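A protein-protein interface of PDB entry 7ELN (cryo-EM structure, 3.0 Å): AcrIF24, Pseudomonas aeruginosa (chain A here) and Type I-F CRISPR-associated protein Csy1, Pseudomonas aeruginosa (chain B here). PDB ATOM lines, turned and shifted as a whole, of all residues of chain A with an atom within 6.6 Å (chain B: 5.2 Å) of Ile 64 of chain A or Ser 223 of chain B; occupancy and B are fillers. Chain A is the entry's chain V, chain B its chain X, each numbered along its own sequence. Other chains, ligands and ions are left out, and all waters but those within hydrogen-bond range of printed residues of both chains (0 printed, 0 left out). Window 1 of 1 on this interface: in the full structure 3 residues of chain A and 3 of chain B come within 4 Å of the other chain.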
ATOM      1  N   SER A  56      17.804  26.109 -21.726  1.00  0.00           N
ATOM      2  CA  SER A  56      18.981  26.112 -22.587  1.00  0.00           C
ATOM      3  C   SER A  56      20.109  26.978 -22.046  1.00  0.00           C
ATOM      4  O   SER A  56      21.282  26.651 -22.245  1.00  0.00           O
ATOM      5  CB  SER A  56      18.591  26.587 -23.979  1.00  0.00           C
ATOM      6  OG  SER A  56      18.637  27.997 -24.037  1.00  0.00           O
ATOM      7  N   ASP A  57      19.783  28.056 -21.333  1.00  0.00           N
ATOM      8  CA  ASP A  57      20.827  28.924 -20.801  1.00  0.00           C
ATOM      9  C   ASP A  57      21.585  28.258 -19.662  1.00  0.00           C
ATOM     10  O   ASP A  57      22.814  28.362 -19.588  1.00  0.00           O
ATOM     11  CB  ASP A  57      20.221  30.239 -20.333  1.00  0.00           C
ATOM     12  CG  ASP A  57      20.135  31.256 -21.439  1.00  0.00           C
ATOM     13  OD1 ASP A  57      20.820  31.070 -22.464  1.00  0.00           O
ATOM     14  OD2 ASP A  57      19.386  32.242 -21.288  1.00  0.00           O
ATOM     15  N   ILE A  59      21.856  25.023 -19.261  1.00  0.00           N
ATOM     16  CA  ILE A  59      22.613  23.947 -19.894  1.00  0.00           C
ATOM     17  C   ILE A  59      23.885  24.492 -20.537  1.00  0.00           C
ATOM     18  O   ILE A  59      24.967  23.899 -20.416  1.00  0.00           O
ATOM     19  CB  ILE A  59      21.717  23.220 -20.909  1.00  0.00           C
ATOM     20  CG1 ILE A  59      20.641  22.436 -20.174  1.00  0.00           C
ATOM     21  CG2 ILE A  59      22.514  22.302 -21.792  1.00  0.00           C
ATOM     22  CD1 ILE A  59      19.653  21.788 -21.076  1.00  0.00           C
ATOM     23  N   ALA A  60      23.789  25.662 -21.162  1.00  0.00           N
ATOM     24  CA  ALA A  60      24.946  26.259 -21.812  1.00  0.00           C
ATOM     25  C   ALA A  60      25.988  26.717 -20.802  1.00  0.00           C
ATOM     26  O   ALA A  60      27.192  26.582 -21.047  1.00  0.00           O
ATOM     27  CB  ALA A  60      24.497  27.425 -22.676  1.00  0.00           C
ATOM     28  N   GLU A  61      25.552  27.246 -19.659  1.00  0.00           N
ATOM     29  CA  GLU A  61      26.512  27.630 -18.630  1.00  0.00           C
ATOM     30  C   GLU A  61      27.167  26.413 -17.995  1.00  0.00           C
ATOM     31  O   GLU A  61      28.339  26.475 -17.603  1.00  0.00           O
ATOM     32  CB  GLU A  61      25.844  28.478 -17.561  1.00  0.00           C
ATOM     33  CG  GLU A  61      25.305  29.785 -18.062  1.00  0.00           C
ATOM     34  CD  GLU A  61      24.560  30.531 -16.984  1.00  0.00           C
ATOM     35  OE1 GLU A  61      24.657  30.117 -15.809  1.00  0.00           O
ATOM     36  OE2 GLU A  61      23.870  31.521 -17.306  1.00  0.00           O
ATOM     37  N   PHE A  62      26.431  25.301 -17.887  1.00  0.00           N
ATOM     38  CA  PHE A  62      27.049  24.052 -17.454  1.00  0.00           C
ATOM     39  C   PHE A  62      28.129  23.611 -18.425  1.00  0.00           C
ATOM     40  O   PHE A  62      29.196  23.152 -18.005  1.00  0.00           O
ATOM     41  CB  PHE A  62      26.004  22.950 -17.318  1.00  0.00           C
ATOM     42  CG  PHE A  62      26.563  21.650 -16.825  1.00  0.00           C
ATOM     43  CD1 PHE A  62      26.754  21.448 -15.481  1.00  0.00           C
ATOM     44  CD2 PHE A  62      26.891  20.631 -17.700  1.00  0.00           C
ATOM     45  CE1 PHE A  62      27.263  20.266 -15.019  1.00  0.00           C
ATOM     46  CE2 PHE A  62      27.403  19.453 -17.240  1.00  0.00           C
ATOM     47  CZ  PHE A  62      27.586  19.270 -15.900  1.00  0.00           C
ATOM     48  N   VAL A  63      27.856  23.725 -19.723  1.00  0.00           N
ATOM     49  CA  VAL A  63      28.829  23.326 -20.734  1.00  0.00           C
ATOM     50  C   VAL A  63      30.058  24.220 -20.680  1.00  0.00           C
ATOM     51  O   VAL A  63      31.190  23.737 -20.772  1.00  0.00           O
ATOM     52  CB  VAL A  63      28.170  23.333 -22.123  1.00  0.00           C
ATOM     53  CG1 VAL A  63      29.190  23.211 -23.225  1.00  0.00           C
ATOM     54  CG2 VAL A  63      27.197  22.199 -22.219  1.00  0.00           C
ATOM     55  N   ILE A  64      29.856  25.522 -20.464  1.00  0.00           N
ATOM     56  CA  ILE A  64      30.966  26.470 -20.363  1.00  0.00           C
ATOM     57  C   ILE A  64      31.844  26.154 -19.160  1.00  0.00           C
ATOM     58  O   ILE A  64      33.077  26.095 -19.272  1.00  0.00           O
ATOM     59  CB  ILE A  64      30.420  27.906 -20.300  1.00  0.00           C
ATOM     60  CG1 ILE A  64      29.919  28.341 -21.665  1.00  0.00           C
ATOM     61  CG2 ILE A  64      31.472  28.871 -19.821  1.00  0.00           C
ATOM     62  CD1 ILE A  64      30.990  28.366 -22.695  1.00  0.00           C
ATOM     63  N   ASP A  65      31.226  25.901 -18.006  1.00  0.00           N
ATOM     64  CA  ASP A  65      32.006  25.610 -16.808  1.00  0.00           C
ATOM     65  C   ASP A  65      32.715  24.269 -16.905  1.00  0.00           C
ATOM     66  O   ASP A  65      33.859  24.143 -16.462  1.00  0.00           O
ATOM     67  CB  ASP A  65      31.118  25.626 -15.574  1.00  0.00           C
ATOM     68  CG  ASP A  65      31.902  25.381 -14.307  1.00  0.00           C
ATOM     69  OD1 ASP A  65      32.569  26.321 -13.826  1.00  0.00           O
ATOM     70  OD2 ASP A  65      31.855  24.251 -13.784  1.00  0.00           O
ATOM     71  N   ALA A  66      32.063  23.257 -17.479  1.00  0.00           N
ATOM     72  CA  ALA A  66      32.703  21.954 -17.593  1.00  0.00           C
ATOM     73  C   ALA A  66      33.792  21.957 -18.649  1.00  0.00           C
ATOM     74  O   ALA A  66      34.754  21.193 -18.547  1.00  0.00           O
ATOM     75  CB  ALA A  66      31.666  20.886 -17.908  1.00  0.00           C
ATOM     76  N   ARG A  67      33.663  22.808 -19.659  1.00  0.00           N
ATOM     77  CA  ARG A  67      34.709  22.929 -20.657  1.00  0.00           C
ATOM     78  C   ARG A  67      35.916  23.653 -20.099  1.00  0.00           C
ATOM     79  O   ARG A  67      37.053  23.284 -20.404  1.00  0.00           O
ATOM     80  CB  ARG A  67      34.165  23.665 -21.870  1.00  0.00           C
ATOM     81  CG  ARG A  67      35.101  23.711 -23.025  1.00  0.00           C
ATOM     82  CD  ARG A  67      34.316  23.744 -24.296  1.00  0.00           C
ATOM     83  NE  ARG A  67      33.443  24.902 -24.347  1.00  0.00           N
ATOM     84  CZ  ARG A  67      32.419  25.019 -25.181  1.00  0.00           C
ATOM     85  NH1 ARG A  67      32.137  24.039 -26.024  1.00  0.00           N
ATOM     86  NH2 ARG A  67      31.673  26.113 -25.170  1.00  0.00           N
ATOM     87  N   HIS A  68      35.699  24.673 -19.277  1.00  0.00           N
ATOM     88  CA  HIS A  68      36.828  25.388 -18.701  1.00  0.00           C
ATOM     89  C   HIS A  68      37.481  24.607 -17.572  1.00  0.00           C
ATOM     90  O   HIS A  68      38.698  24.686 -17.397  1.00  0.00           O
ATOM     91  CB  HIS A  68      36.371  26.761 -18.216  1.00  0.00           C
ATOM     92  CG  HIS A  68      37.371  27.467 -17.360  1.00  0.00           C
ATOM     93  ND1 HIS A  68      37.367  27.381 -15.984  1.00  0.00           N
ATOM     94  CD2 HIS A  68      38.408  28.275 -17.683  1.00  0.00           C
ATOM     95  CE1 HIS A  68      38.359  28.104 -15.498  1.00  0.00           C
ATOM     96  NE2 HIS A  68      39.006  28.656 -16.507  1.00  0.00           N
ATOM     97  N   ARG A  69      36.701  23.842 -16.813  1.00  0.00           N
ATOM     98  CA  ARG A  69      37.239  23.154 -15.648  1.00  0.00           C
ATOM     99  C   ARG A  69      38.099  21.970 -16.046  1.00  0.00           C
ATOM    100  O   ARG A  69      39.188  21.773 -15.500  1.00  0.00           O
ATOM    101  CB  ARG A  69      36.096  22.695 -14.749  1.00  0.00           C
ATOM    102  CG  ARG A  69      36.529  21.854 -13.575  1.00  0.00           C
ATOM    103  CD  ARG A  69      35.331  21.273 -12.864  1.00  0.00           C
ATOM    104  NE  ARG A  69      34.264  22.255 -12.729  1.00  0.00           N
ATOM    105  CZ  ARG A  69      34.171  23.123 -11.730  1.00  0.00           C
ATOM    106  NH1 ARG A  69      35.082  23.130 -10.768  1.00  0.00           N
ATOM    107  NH2 ARG A  69      33.168  23.984 -11.689  1.00  0.00           N
ATOM    108  N   ARG B 219      22.875  32.975 -31.685  1.00  0.00           N
ATOM    109  CA  ARG B 219      22.617  32.971 -30.248  1.00  0.00           C
ATOM    110  C   ARG B 219      23.136  31.697 -29.593  1.00  0.00           C
ATOM    111  O   ARG B 219      23.683  31.742 -28.485  1.00  0.00           O
ATOM    112  CB  ARG B 219      21.124  33.126 -29.981  1.00  0.00           C
ATOM    113  CG  ARG B 219      20.659  34.550 -30.053  1.00  0.00           C
ATOM    114  CD  ARG B 219      19.204  34.702 -29.689  1.00  0.00           C
ATOM    115  NE  ARG B 219      18.826  36.109 -29.695  1.00  0.00           N
ATOM    116  CZ  ARG B 219      18.211  36.706 -30.708  1.00  0.00           C
ATOM    117  NH1 ARG B 219      17.899  36.011 -31.790  1.00  0.00           N
ATOM    118  NH2 ARG B 219      17.908  37.994 -30.637  1.00  0.00           N
ATOM    119  N   GLU B 220      22.966  30.551 -30.256  1.00  0.00           N
ATOM    120  CA  GLU B 220      23.544  29.315 -29.742  1.00  0.00           C
ATOM    121  C   GLU B 220      25.065  29.344 -29.850  1.00  0.00           C
ATOM    122  O   GLU B 220      25.766  28.750 -29.026  1.00  0.00           O
ATOM    123  CB  GLU B 220      22.995  28.105 -30.499  1.00  0.00           C
ATOM    124  CG  GLU B 220      21.482  27.835 -30.363  1.00  0.00           C
ATOM    125  CD  GLU B 220      20.983  27.462 -28.968  1.00  0.00           C
ATOM    126  OE1 GLU B 220      21.787  27.262 -28.028  1.00  0.00           O
ATOM    127  OE2 GLU B 220      19.748  27.353 -28.807  1.00  0.00           O
ATOM    128  N   ALA B 221      25.600  30.038 -30.864  1.00  0.00           N
ATOM    129  CA  ALA B 221      27.045  30.122 -31.024  1.00  0.00           C
ATOM    130  C   ALA B 221      27.669  30.989 -29.945  1.00  0.00           C
ATOM    131  O   ALA B 221      28.831  30.790 -29.589  1.00  0.00           O
ATOM    132  CB  ALA B 221      27.385  30.662 -32.408  1.00  0.00           C
ATOM    133  N   ARG B 222      26.925  31.976 -29.435  1.00  0.00           N
ATOM    134  CA  ARG B 222      27.443  32.770 -28.323  1.00  0.00           C
ATOM    135  C   ARG B 222      27.595  31.932 -27.069  1.00  0.00           C
ATOM    136  O   ARG B 222      28.550  32.109 -26.304  1.00  0.00           O
ATOM    137  CB  ARG B 222      26.539  33.964 -28.049  1.00  0.00           C
ATOM    138  CG  ARG B 222      26.796  35.162 -28.934  1.00  0.00           C
ATOM    139  CD  ARG B 222      28.009  35.996 -28.489  1.00  0.00           C
ATOM    140  NE  ARG B 222      29.313  35.455 -28.885  1.00  0.00           N
ATOM    141  CZ  ARG B 222      29.818  35.492 -30.115  1.00  0.00           C
ATOM    142  NH1 ARG B 222      29.151  36.057 -31.112  1.00  0.00           N
ATOM    143  NH2 ARG B 222      31.012  34.968 -30.344  1.00  0.00           N
ATOM    144  N   SER B 223      26.658  31.019 -26.839  1.00  0.00           N
ATOM    145  CA  SER B 223      26.780  30.108 -25.711  1.00  0.00           C
ATOM    146  C   SER B 223      27.879  29.080 -25.945  1.00  0.00           C
ATOM    147  O   SER B 223      28.651  28.766 -25.032  1.00  0.00           O
ATOM    148  CB  SER B 223      25.440  29.433 -25.474  1.00  0.00           C
ATOM    149  OG  SER B 223      25.107  28.640 -26.592  1.00  0.00           O
ATOM    150  N   ARG B 224      27.968  28.556 -27.168  1.00  0.00           N
ATOM    151  CA  ARG B 224      28.987  27.567 -27.500  1.00  0.00           C
ATOM    152  C   ARG B 224      30.376  28.191 -27.573  1.00  0.00           C
ATOM    153  O   ARG B 224      31.386  27.481 -27.469  1.00  0.00           O
ATOM    154  CB  ARG B 224      28.649  26.907 -28.832  1.00  0.00           C
ATOM    155  CG  ARG B 224      27.472  25.976 -28.808  1.00  0.00           C
ATOM    156  CD  ARG B 224      27.717  24.802 -27.893  1.00  0.00           C
ATOM    157  NE  ARG B 224      26.475  24.324 -27.313  1.00  0.00           N
ATOM    158  CZ  ARG B 224      26.010  24.740 -26.144  1.00  0.00           C
ATOM    159  NH1 ARG B 224      26.678  25.655 -25.459  1.00  0.00           N
ATOM    160  NH2 ARG B 224      24.874  24.257 -25.671  1.00  0.00           N
ATOM    161  N   GLN B 225      30.436  29.510 -27.794  1.00  0.00           N
ATOM    162  CA  GLN B 225      31.646  30.336 -27.892  1.00  0.00           C
ATOM    163  C   GLN B 225      32.541  29.923 -29.055  1.00  0.00           C
ATOM    164  O   GLN B 225      33.733  30.249 -29.064  1.00  0.00           O
ATOM    165  CB  GLN B 225      32.459  30.331 -26.593  1.00  0.00           C
ATOM    166  CG  GLN B 225      31.678  30.747 -25.362  1.00  0.00           C
ATOM    167  CD  GLN B 225      32.205  32.006 -24.708  1.00  0.00           C
ATOM    168  OE1 GLN B 225      33.122  32.650 -25.213  1.00  0.00           O
ATOM    169  NE2 GLN B 225      31.641  32.348 -23.557  1.00  0.00           N
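Of the printed residues of chain B, Ala 60 of chain A touches Ser 223 and Arg 224. Ile 64 of chain A touches two residues of chain B. Of the printed residues of chain B, Arg 67 of chain A touches Arg 224. Arg 69 of chain A touches none of the printed residues of chain B. Glu 220 of chain B touches none of the printed residues of chain A. Of chain A, only Ala 60 and Ile 64 come within 4 Å of Ser 223 of chain B. Of the printed residues of chain A, Arg 224 of chain B touches Ala 60 (3.95 Å) and Arg 67 (2.7 Å). Of the printed residues of chain A, Gln 225 of chain B touches Ile 64. The nearest residue of chain B that does not touch Ile 64 of chain A is Arg 224 of chain B (4.9 Å). The nearest residue of chain A that does not touch Ser 223 of chain B is Arg 67 of chain A (4.02 Å).
Among the printed residues, pairs that only touch across the chains: Ala 60 of chain A with Ser 223 of chain B, Ala 60 of chain A with Arg 224 of chain B, Ile 64 of chain A with Ser 223 of chain B and Ile 64 of chain A with Gln 225 of chain B.
O of Arg 224 of chain B lies within hydrogen-bond range of NH2 of Arg 67 of chain A.
The backbone carbonyl oxygen (O) of Glu 220 of chain B lies within hydrogen-bond range of the side-chain hydroxyl (OG) of Ser 223 of chain B (2.5 Å).
Of the 13 printed residues of chain A, 3 touch a printed residue of chain B. Printed residues of chain A that touch a printed residue of chain B: Ala 60, Ile 64 and Arg 67. Along chain A the printed residues that touch a printed residue of chain B span positions 60 to 67. Of the 7 printed residues of chain B, 3 touch a printed residue of chain A.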
